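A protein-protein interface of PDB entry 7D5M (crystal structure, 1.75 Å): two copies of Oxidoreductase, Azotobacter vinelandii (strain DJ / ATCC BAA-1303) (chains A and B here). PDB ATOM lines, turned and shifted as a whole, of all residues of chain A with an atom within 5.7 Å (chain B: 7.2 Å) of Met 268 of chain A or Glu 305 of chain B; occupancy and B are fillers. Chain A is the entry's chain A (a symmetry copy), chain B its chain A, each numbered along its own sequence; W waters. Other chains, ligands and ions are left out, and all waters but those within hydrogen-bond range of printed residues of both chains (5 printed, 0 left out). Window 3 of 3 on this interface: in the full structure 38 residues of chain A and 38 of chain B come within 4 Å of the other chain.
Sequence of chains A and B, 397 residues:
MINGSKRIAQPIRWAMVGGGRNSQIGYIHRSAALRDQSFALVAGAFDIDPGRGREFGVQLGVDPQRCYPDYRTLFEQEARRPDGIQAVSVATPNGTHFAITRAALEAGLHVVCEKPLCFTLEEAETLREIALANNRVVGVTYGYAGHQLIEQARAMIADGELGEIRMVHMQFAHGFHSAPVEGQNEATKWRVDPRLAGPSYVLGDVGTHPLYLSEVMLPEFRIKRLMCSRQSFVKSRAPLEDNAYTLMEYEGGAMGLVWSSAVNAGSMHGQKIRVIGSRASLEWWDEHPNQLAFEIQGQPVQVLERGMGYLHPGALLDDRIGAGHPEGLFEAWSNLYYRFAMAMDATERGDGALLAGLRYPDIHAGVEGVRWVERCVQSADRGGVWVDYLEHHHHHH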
ATOM      1  N   ALA A 173      -9.047  -8.352  22.085  1.00  0.00           N
ATOM      2  CA  ALA A 173      -7.685  -8.809  21.739  1.00  0.00           C
ATOM      3  C   ALA A 173      -7.653 -10.334  21.765  1.00  0.00           C
ATOM      4  O   ALA A 173      -7.448 -10.914  22.839  1.00  0.00           O
ATOM      5  CB  ALA A 173      -6.687  -8.211  22.701  1.00  0.00           C
ATOM      6  N   HIS A 174      -7.883 -10.950  20.606  1.00  0.00           N
ATOM      7  CA  HIS A 174      -7.838 -12.416  20.398  1.00  0.00           C
ATOM      8  C   HIS A 174      -6.596 -12.763  19.571  1.00  0.00           C
ATOM      9  O   HIS A 174      -5.962 -11.848  19.030  1.00  0.00           O
ATOM     10  CB  HIS A 174      -9.133 -12.906  19.743  1.00  0.00           C
ATOM     11  CG  HIS A 174      -9.273 -12.497  18.320  1.00  0.00           C
ATOM     12  ND1 HIS A 174      -8.708 -13.223  17.285  1.00  0.00           N
ATOM     13  CD2 HIS A 174      -9.911 -11.453  17.757  1.00  0.00           C
ATOM     14  CE1 HIS A 174      -9.000 -12.633  16.136  1.00  0.00           C
ATOM     15  NE2 HIS A 174      -9.759 -11.558  16.402  1.00  0.00           N
ATOM     16  N   GLY A 175      -6.258 -14.049  19.495  1.00  0.00           N
ATOM     17  CA  GLY A 175      -5.016 -14.496  18.848  1.00  0.00           C
ATOM     18  C   GLY A 175      -5.268 -15.311  17.595  1.00  0.00           C
ATOM     19  O   GLY A 175      -4.299 -15.865  17.065  1.00  0.00           O
ATOM     20  N   PHE A 176      -6.505 -15.406  17.105  1.00  0.00           N
ATOM     21  CA  PHE A 176      -6.807 -16.377  16.020  1.00  0.00           C
ATOM     22  C   PHE A 176      -6.042 -16.042  14.743  1.00  0.00           C
ATOM     23  O   PHE A 176      -5.844 -16.984  13.968  1.00  0.00           O
ATOM     24  CB  PHE A 176      -8.299 -16.490  15.726  1.00  0.00           C
ATOM     25  CG  PHE A 176      -9.035 -17.214  16.824  1.00  0.00           C
ATOM     26  CD1 PHE A 176      -8.917 -18.582  16.987  1.00  0.00           C
ATOM     27  CD2 PHE A 176      -9.817 -16.506  17.714  1.00  0.00           C
ATOM     28  CE1 PHE A 176      -9.584 -19.231  18.017  1.00  0.00           C
ATOM     29  CE2 PHE A 176     -10.500 -17.158  18.728  1.00  0.00           C
ATOM     30  CZ  PHE A 176     -10.368 -18.516  18.887  1.00  0.00           C
ATOM     31  N   GLY A 266      -2.839 -16.878  21.931  1.00  0.00           N
ATOM     32  CA  GLY A 266      -3.344 -17.641  23.088  1.00  0.00           C
ATOM     33  C   GLY A 266      -4.678 -17.122  23.601  1.00  0.00           C
ATOM     34  O   GLY A 266      -5.358 -17.876  24.332  1.00  0.00           O
ATOM     35  N   SER A 267      -5.057 -15.890  23.260  1.00  0.00           N
ATOM     36  CA  SER A 267      -6.339 -15.291  23.714  1.00  0.00           C
ATOM     37  C   SER A 267      -7.491 -15.880  22.892  1.00  0.00           C
ATOM     38  O   SER A 267      -7.458 -15.805  21.658  1.00  0.00           O
ATOM     39  CB  SER A 267      -6.338 -13.791  23.635  1.00  0.00           C
ATOM     40  OG  SER A 267      -7.626 -13.291  24.001  1.00  0.00           O
ATOM     41  N   MET A 268      -8.503 -16.392  23.580  1.00  0.00           N
ATOM     42  CA  MET A 268      -9.712 -17.001  22.972  1.00  0.00           C
ATOM     43  C   MET A 268     -10.669 -15.911  22.476  1.00  0.00           C
ATOM     44  O   MET A 268     -11.428 -16.173  21.534  1.00  0.00           O
ATOM     45  CB  MET A 268     -10.405 -17.897  24.003  1.00  0.00           C
ATOM     46  CG  MET A 268      -9.634 -19.174  24.296  1.00  0.00           C
ATOM     47  SD  MET A 268      -9.402 -20.189  22.809  1.00  0.00           S
ATOM     48  CE  MET A 268     -11.099 -20.427  22.306  1.00  0.00           C
ATOM     49  N   HIS A 269     -10.659 -14.723  23.078  1.00  0.00           N
ATOM     50  CA  HIS A 269     -11.553 -13.612  22.661  1.00  0.00           C
ATOM     51  C   HIS A 269     -11.061 -12.311  23.278  1.00  0.00           C
ATOM     52  O   HIS A 269     -10.710 -11.396  22.528  1.00  0.00           O
ATOM     53  CB  HIS A 269     -13.012 -13.913  23.027  1.00  0.00           C
ATOM     54  CG  HIS A 269     -13.946 -13.832  21.870  1.00  0.00           C
ATOM     55  ND1 HIS A 269     -15.108 -13.084  21.908  1.00  0.00           N
ATOM     56  CD2 HIS A 269     -13.912 -14.421  20.654  1.00  0.00           C
ATOM     57  CE1 HIS A 269     -15.743 -13.212  20.763  1.00  0.00           C
ATOM     58  NE2 HIS A 269     -15.022 -14.022  19.967  1.00  0.00           N
ATOM     59  N   GLY A 270     -11.032 -12.258  24.606  1.00  0.00           N
ATOM     60  CA  GLY A 270     -10.394 -11.162  25.352  1.00  0.00           C
ATOM     61  C   GLY A 270     -11.100  -9.850  25.102  1.00  0.00           C
ATOM     62  O   GLY A 270     -10.414  -8.844  24.929  1.00  0.00           O
ATOM     63  N   GLU A 287     -16.312 -13.458  27.643  1.00  0.00           N
ATOM     64  CA  GLU A 287     -16.216 -14.940  27.696  1.00  0.00           C
ATOM     65  C   GLU A 287     -16.944 -15.460  28.942  1.00  0.00           C
ATOM     66  O   GLU A 287     -17.234 -16.654  29.004  1.00  0.00           O
ATOM     67  CB  GLU A 287     -14.758 -15.392  27.663  1.00  0.00           C
ATOM     68  CG  GLU A 287     -14.068 -15.070  26.351  1.00  0.00           C
ATOM     69  CD  GLU A 287     -12.590 -15.403  26.371  1.00  0.00           C
ATOM     70  OE1 GLU A 287     -12.252 -16.601  26.546  1.00  0.00           O
ATOM     71  OE2 GLU A 287     -11.789 -14.462  26.288  1.00  0.00           O
ATOM     72  N   LEU B 149     -18.390 -30.178  25.778  1.00  0.00           N
ATOM     73  CA  LEU B 149     -17.152 -30.632  26.464  1.00  0.00           C
ATOM     74  C   LEU B 149     -17.424 -31.865  27.326  1.00  0.00           C
ATOM     75  O   LEU B 149     -16.437 -32.502  27.739  1.00  0.00           O
ATOM     76  CB  LEU B 149     -16.534 -29.484  27.260  1.00  0.00           C
ATOM     77  CG  LEU B 149     -15.856 -28.424  26.399  1.00  0.00           C
ATOM     78  CD1 LEU B 149     -15.415 -27.257  27.259  1.00  0.00           C
ATOM     79  CD2 LEU B 149     -14.672 -29.007  25.631  1.00  0.00           C
ATOM     80  N   ASN B 290     -18.060 -23.771  28.880  1.00  0.00           N
ATOM     81  CA  ASN B 290     -17.259 -23.725  27.631  1.00  0.00           C
ATOM     82  C   ASN B 290     -15.787 -24.044  27.891  1.00  0.00           C
ATOM     83  O   ASN B 290     -15.025 -23.998  26.927  1.00  0.00           O
ATOM     84  CB  ASN B 290     -17.414 -22.370  26.945  1.00  0.00           C
ATOM     85  CG  ASN B 290     -18.869 -22.066  26.685  1.00  0.00           C
ATOM     86  OD1 ASN B 290     -19.578 -22.877  26.084  1.00  0.00           O
ATOM     87  ND2 ASN B 290     -19.323 -20.910  27.151  1.00  0.00           N
ATOM     88  N   GLN B 291     -15.408 -24.356  29.135  1.00  0.00           N
ATOM     89  CA  GLN B 291     -14.022 -24.736  29.499  1.00  0.00           C
ATOM     90  C   GLN B 291     -14.035 -26.097  30.186  1.00  0.00           C
ATOM     91  O   GLN B 291     -15.036 -26.443  30.845  1.00  0.00           O
ATOM     92  CB  GLN B 291     -13.364 -23.680  30.385  1.00  0.00           C
ATOM     93  CG  GLN B 291     -13.057 -22.389  29.632  1.00  0.00           C
ATOM     94  CD  GLN B 291     -14.258 -21.483  29.525  1.00  0.00           C
ATOM     95  OE1 GLN B 291     -15.001 -21.311  30.491  1.00  0.00           O
ATOM     96  NE2 GLN B 291     -14.450 -20.879  28.360  1.00  0.00           N
ATOM     97  N   LEU B 292     -12.957 -26.845  30.009  1.00  0.00           N
ATOM     98  CA  LEU B 292     -12.749 -28.142  30.690  1.00  0.00           C
ATOM     99  C   LEU B 292     -11.299 -28.192  31.168  1.00  0.00           C
ATOM    100  O   LEU B 292     -10.382 -28.093  30.318  1.00  0.00           O
ATOM    101  CB  LEU B 292     -13.076 -29.272  29.717  1.00  0.00           C
ATOM    102  CG  LEU B 292     -12.851 -30.687  30.256  1.00  0.00           C
ATOM    103  CD1 LEU B 292     -13.905 -31.044  31.285  1.00  0.00           C
ATOM    104  CD2 LEU B 292     -12.859 -31.684  29.113  1.00  0.00           C
ATOM    105  N   VAL B 303      -6.416 -25.841  30.048  1.00  0.00           N
ATOM    106  CA  VAL B 303      -7.872 -25.584  29.912  1.00  0.00           C
ATOM    107  C   VAL B 303      -8.246 -25.853  28.456  1.00  0.00           C
ATOM    108  O   VAL B 303      -7.662 -25.233  27.562  1.00  0.00           O
ATOM    109  CB  VAL B 303      -8.228 -24.157  30.354  1.00  0.00           C
ATOM    110  CG1 VAL B 303      -9.683 -23.837  30.062  1.00  0.00           C
ATOM    111  CG2 VAL B 303      -7.931 -23.939  31.827  1.00  0.00           C
ATOM    112  N   LEU B 304      -9.182 -26.768  28.238  1.00  0.00           N
ATOM    113  CA  LEU B 304      -9.694 -27.062  26.883  1.00  0.00           C
ATOM    114  C   LEU B 304     -10.903 -26.160  26.649  1.00  0.00           C
ATOM    115  O   LEU B 304     -11.742 -26.057  27.561  1.00  0.00           O
ATOM    116  CB  LEU B 304     -10.093 -28.532  26.772  1.00  0.00           C
ATOM    117  CG  LEU B 304      -9.079 -29.550  27.275  1.00  0.00           C
ATOM    118  CD1 LEU B 304      -9.525 -30.955  26.911  1.00  0.00           C
ATOM    119  CD2 LEU B 304      -7.695 -29.290  26.723  1.00  0.00           C
ATOM    120  N   GLU B 305     -10.981 -25.559  25.468  1.00  0.00           N
ATOM    121  CA  GLU B 305     -12.023 -24.576  25.097  1.00  0.00           C
ATOM    122  C   GLU B 305     -12.961 -25.180  24.060  1.00  0.00           C
ATOM    123  O   GLU B 305     -12.470 -25.786  23.089  1.00  0.00           O
ATOM    124  CB  GLU B 305     -11.372 -23.311  24.542  1.00  0.00           C
ATOM    125  CG  GLU B 305     -10.771 -22.440  25.625  1.00  0.00           C
ATOM    126  CD  GLU B 305     -11.698 -21.403  26.236  1.00  0.00           C
ATOM    127  OE1 GLU B 305     -12.843 -21.269  25.765  1.00  0.00           O
ATOM    128  OE2 GLU B 305     -11.254 -20.719  27.195  1.00  0.00           O
ATOM    129  N   ARG B 306     -14.260 -24.960  24.244  1.00  0.00           N
ATOM    130  CA  ARG B 306     -15.303 -25.288  23.243  1.00  0.00           C
ATOM    131  C   ARG B 306     -14.877 -24.748  21.880  1.00  0.00           C
ATOM    132  O   ARG B 306     -14.422 -23.572  21.799  1.00  0.00           O
ATOM    133  CB  ARG B 306     -16.631 -24.647  23.636  1.00  0.00           C
ATOM    134  CG  ARG B 306     -17.818 -25.078  22.791  1.00  0.00           C
ATOM    135  CD  ARG B 306     -18.967 -24.092  22.942  1.00  0.00           C
ATOM    136  NE  ARG B 306     -18.658 -22.758  22.449  1.00  0.00           N
ATOM    137  CZ  ARG B 306     -18.566 -22.408  21.165  1.00  0.00           C
ATOM    138  NH1 ARG B 306     -18.740 -23.307  20.203  1.00  0.00           N
ATOM    139  NH2 ARG B 306     -18.290 -21.155  20.845  1.00  0.00           N
ATOM    140  N   GLY B 307     -15.046 -25.551  20.832  1.00  0.00           N
ATOM    141  CA  GLY B 307     -14.900 -25.080  19.443  1.00  0.00           C
ATOM    142  C   GLY B 307     -13.476 -25.150  18.909  1.00  0.00           C
ATOM    143  O   GLY B 307     -13.284 -24.801  17.731  1.00  0.00           O
ATOM    144  N   MET B 308     -12.499 -25.607  19.691  1.00  0.00           N
ATOM    145  CA  MET B 308     -11.084 -25.606  19.232  1.00  0.00           C
ATOM    146  C   MET B 308     -10.751 -26.903  18.486  1.00  0.00           C
ATOM    147  O   MET B 308     -11.282 -27.969  18.833  1.00  0.00           O
ATOM    148  CB  MET B 308     -10.117 -25.394  20.394  1.00  0.00           C
ATOM    149  CG  MET B 308     -10.168 -23.981  20.943  1.00  0.00           C
ATOM    150  SD  MET B 308      -9.728 -22.696  19.744  1.00  0.00           S
ATOM    151  CE  MET B 308      -7.944 -22.863  19.756  1.00  0.00           C
ATOM    152  N   GLY B 309      -9.849 -26.800  17.508  1.00  0.00           N
ATOM    153  CA  GLY B 309      -9.500 -27.903  16.589  1.00  0.00           C
ATOM    154  C   GLY B 309      -8.817 -29.083  17.263  1.00  0.00           C
ATOM    155  O   GLY B 309      -8.821 -30.179  16.674  1.00  0.00           O
ATOM    156  N   TYR B 310      -8.247 -28.903  18.457  1.00  0.00           N
ATOM    157  CA  TYR B 310      -7.598 -29.987  19.239  1.00  0.00           C
ATOM    158  C   TYR B 310      -8.635 -30.888  19.924  1.00  0.00           C
ATOM    159  O   TYR B 310      -8.221 -31.908  20.495  1.00  0.00           O
ATOM    160  CB  TYR B 310      -6.597 -29.422  20.249  1.00  0.00           C
ATOM    161  CG  TYR B 310      -7.128 -28.364  21.186  1.00  0.00           C
ATOM    162  CD1 TYR B 310      -8.053 -28.673  22.173  1.00  0.00           C
ATOM    163  CD2 TYR B 310      -6.673 -27.055  21.107  1.00  0.00           C
ATOM    164  CE1 TYR B 310      -8.552 -27.698  23.020  1.00  0.00           C
ATOM    165  CE2 TYR B 310      -7.140 -26.070  21.967  1.00  0.00           C
ATOM    166  CZ  TYR B 310      -8.081 -26.401  22.931  1.00  0.00           C
ATOM    167  OH  TYR B 310      -8.547 -25.442  23.775  1.00  0.00           O
ATOM    168  N   LEU B 311      -9.928 -30.541  19.893  1.00  0.00           N
ATOM    169  CA  LEU B 311     -10.985 -31.371  20.531  1.00  0.00           C
ATOM    170  C   LEU B 311     -11.256 -32.605  19.671  1.00  0.00           C
ATOM    171  O   LEU B 311     -11.069 -32.545  18.441  1.00  0.00           O
ATOM    172  CB  LEU B 311     -12.286 -30.577  20.704  1.00  0.00           C
ATOM    173  CG  LEU B 311     -12.208 -29.351  21.611  1.00  0.00           C
ATOM    174  CD1 LEU B 311     -13.531 -28.605  21.603  1.00  0.00           C
ATOM    175  CD2 LEU B 311     -11.824 -29.737  23.034  1.00  0.00           C
ATOM    176  N   LEU B 316     -17.065 -31.310  18.497  1.00  0.00           N
ATOM    177  CA  LEU B 316     -17.143 -30.123  17.598  1.00  0.00           C
ATOM    178  C   LEU B 316     -18.458 -30.118  16.807  1.00  0.00           C
ATOM    179  O   LEU B 316     -18.808 -29.065  16.279  1.00  0.00           O
ATOM    180  CB  LEU B 316     -15.933 -30.112  16.655  1.00  0.00           C
ATOM    181  CG  LEU B 316     -14.594 -29.834  17.335  1.00  0.00           C
ATOM    182  CD1 LEU B 316     -13.423 -30.199  16.424  1.00  0.00           C
ATOM    183  CD2 LEU B 316     -14.491 -28.393  17.786  1.00  0.00           C
ATOM    184  N   ASP B 319     -21.159 -27.237  17.582  1.00  0.00           N
ATOM    185  CA  ASP B 319     -20.769 -25.807  17.661  1.00  0.00           C
ATOM    186  C   ASP B 319     -21.710 -24.984  16.774  1.00  0.00           C
ATOM    187  O   ASP B 319     -21.862 -25.333  15.593  1.00  0.00           O
ATOM    188  CB  ASP B 319     -19.308 -25.580  17.286  1.00  0.00           C
ATOM    189  CG  ASP B 319     -18.325 -26.143  18.297  1.00  0.00           C
ATOM    190  OD1 ASP B 319     -18.667 -26.196  19.503  1.00  0.00           O
ATOM    191  OD2 ASP B 319     -17.220 -26.526  17.869  1.00  0.00           O
ATOM    192  N   GLY B 322     -18.243 -19.821  16.467  1.00  0.00           N
ATOM    193  CA  GLY B 322     -16.795 -20.028  16.625  1.00  0.00           C
ATOM    194  C   GLY B 322     -16.345 -19.976  18.070  1.00  0.00           C
ATOM    195  O   GLY B 322     -16.989 -19.287  18.896  1.00  0.00           O
ATOM    196  N   ALA B 323     -15.257 -20.687  18.363  1.00  0.00           N
ATOM    197  CA  ALA B 323     -14.560 -20.704  19.665  1.00  0.00           C
ATOM    198  C   ALA B 323     -14.388 -19.274  20.182  1.00  0.00           C
ATOM    199  O   ALA B 323     -14.143 -18.367  19.353  1.00  0.00           O
ATOM    200  CB  ALA B 323     -13.223 -21.380  19.508  1.00  0.00           C
ATOM    201  N   GLY B 324     -14.527 -19.086  21.499  1.00  0.00           N
ATOM    202  CA  GLY B 324     -14.351 -17.782  22.164  1.00  0.00           C
ATOM    203  C   GLY B 324     -15.664 -17.045  22.374  1.00  0.00           C
ATOM    204  O   GLY B 324     -15.727 -16.233  23.299  1.00  0.00           O
ATOM    205  N   HIS B 325     -16.677 -17.287  21.546  1.00  0.00           N
ATOM    206  CA  HIS B 325     -18.054 -16.783  21.777  1.00  0.00           C
ATOM    207  C   HIS B 325     -18.714 -17.725  22.777  1.00  0.00           C
ATOM    208  O   HIS B 325     -18.768 -18.928  22.521  1.00  0.00           O
ATOM    209  CB  HIS B 325     -18.870 -16.718  20.484  1.00  0.00           C
ATOM    210  CG  HIS B 325     -18.254 -15.933  19.377  1.00  0.00           C
ATOM    211  ND1 HIS B 325     -17.395 -16.500  18.457  1.00  0.00           N
ATOM    212  CD2 HIS B 325     -18.416 -14.647  19.007  1.00  0.00           C
ATOM    213  CE1 HIS B 325     -17.018 -15.574  17.589  1.00  0.00           C
ATOM    214  NE2 HIS B 325     -17.654 -14.439  17.892  1.00  0.00           N
HETATM  215  O   HOH W   1     -13.772 -18.560  25.440  1.00  0.00           O
HETATM  216  O   HOH W   2     -19.247 -18.679  29.631  1.00  0.00           O
HETATM  217  O   HOH W   3      -7.405 -22.999  23.658  1.00  0.00           O
HETATM  218  O   HOH W   4     -16.825 -18.995  27.754  1.00  0.00           O
HETATM  219  O   HOH W   5     -11.320 -18.308  28.196  1.00  0.00           O
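The side-chain carboxylate of Glu 305 of chain B is in hydrogen-bond range of the side-chain amide nitrogen of Gln 291 of chain B, at 3.1 Å. The guanidinium group (NH2) of Arg 306 of chain B sits at hydrogen-bond distance from the backbone carbonyl oxygen (O) of His 325 of chain B, 2.8 Å away. The backbone NH (N) of His 174 of chain A lies within hydrogen-bond range of the backbone carbonyl oxygen (O) of His 269 of chain A (3.4 Å). The backbone NH of His 269 of chain A sits close to the side-chain hydroxyl of Ser 267 of chain A (3.5 Å). The backbone NH of His 269 of chain A lies within hydrogen-bond range of the side-chain carboxylate of Glu 287 of chain A, 3.4 Å away. The side-chain carboxylate of Glu 287 of chain A sits at hydrogen-bond distance from the backbone NH of Gly 270 of chain A (2.9 Å).
O of Gly 324 of chain B sits close to ND1 of His 269 of chain A (3.5 Å). A ring nitrogen (NE2) of His 269 of chain A is in hydrogen-bond range of a ring nitrogen (NE2) of His 325 of chain B, at 3.4 Å.
Among the printed residues, merely in contact across the chains: Met 268 of chain A with Gly 324 of chain B (3.4 Å), Met 268 of chain A with Glu 305 of chain B (3.6 Å), Met 268 of chain A with Ala 323 of chain B (3.6 Å), Glu 287 of chain A with Gly 324 of chain B (3.7 Å), Met 268 of chain A with Met 308 of chain B (3.7 Å), Phe 176 of chain A with Ala 323 of chain B (3.8 Å) and Phe 176 of chain A with Met 308 of chain B (3.9 Å).
No position is printed for both chains.
Of the 10 printed residues of chain A, 4 touch a printed residue of chain B. Hydrophobic or aromatic side chains of chain B within 4 Å of the printed part of chain A: Met 308, Ala 323 and His 325.
Water W5 lies within hydrogen-bond range of OE1 of Glu 287 of chain A and OE2 of Glu 305 of chain B. Water W4 lies within hydrogen-bond range of O of Glu 287 of chain A, NE2 of Gln 291 of chain B and ND2 of Asn 290 of chain B. Water W3 lies within hydrogen-bond range of the side-chain hydroxyl (OH) of Tyr 310 of chain B (2.7 Å) and the side-chain sulfur (SD) of Met 268 of chain A (3.6 Å). Water W1 lies within hydrogen-bond range of the side-chain carboxylate (OE1) of Glu 287 of chain A (2.7 Å) and the side-chain carboxylate (OE1) of Glu 305 of chain B (2.9 Å). Water W2 lies within hydrogen-bond range of the backbone carbonyl oxygen (O) of Glu 287 of chain A and the side-chain amide nitrogen (ND2) of Asn 290 of chain B.
Of chain B, only Glu 305 (3.6 Å), Met 308 (3.7 Å), Ala 323 (3.6 Å) and Gly 324 (3.4 Å) come within 4 Å of Met 268 of chain A. Of the printed residues of chain B, Glu 287 of chain A touches Gly 324. Of the printed residues of chain B, Phe 176 of chain A touches Met 308 and Ala 323. Of the printed residues of chain B, His 269 of chain A touches Gly 324 (3.3 Å) and His 325 (3.4 Å). Printed residues of chain A within 4 Å of Met 308 of chain B: Phe 176 and Met 268. Ala 173 of chain A touches none of the printed residues of chain B. The nearest residue of chain B that does not touch Met 268 of chain A is Arg 306 of chain B (4.6 Å). The nearest printed residue of chain A that does not touch His 325 of chain B is Met 268 of chain A (5.4 Å).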
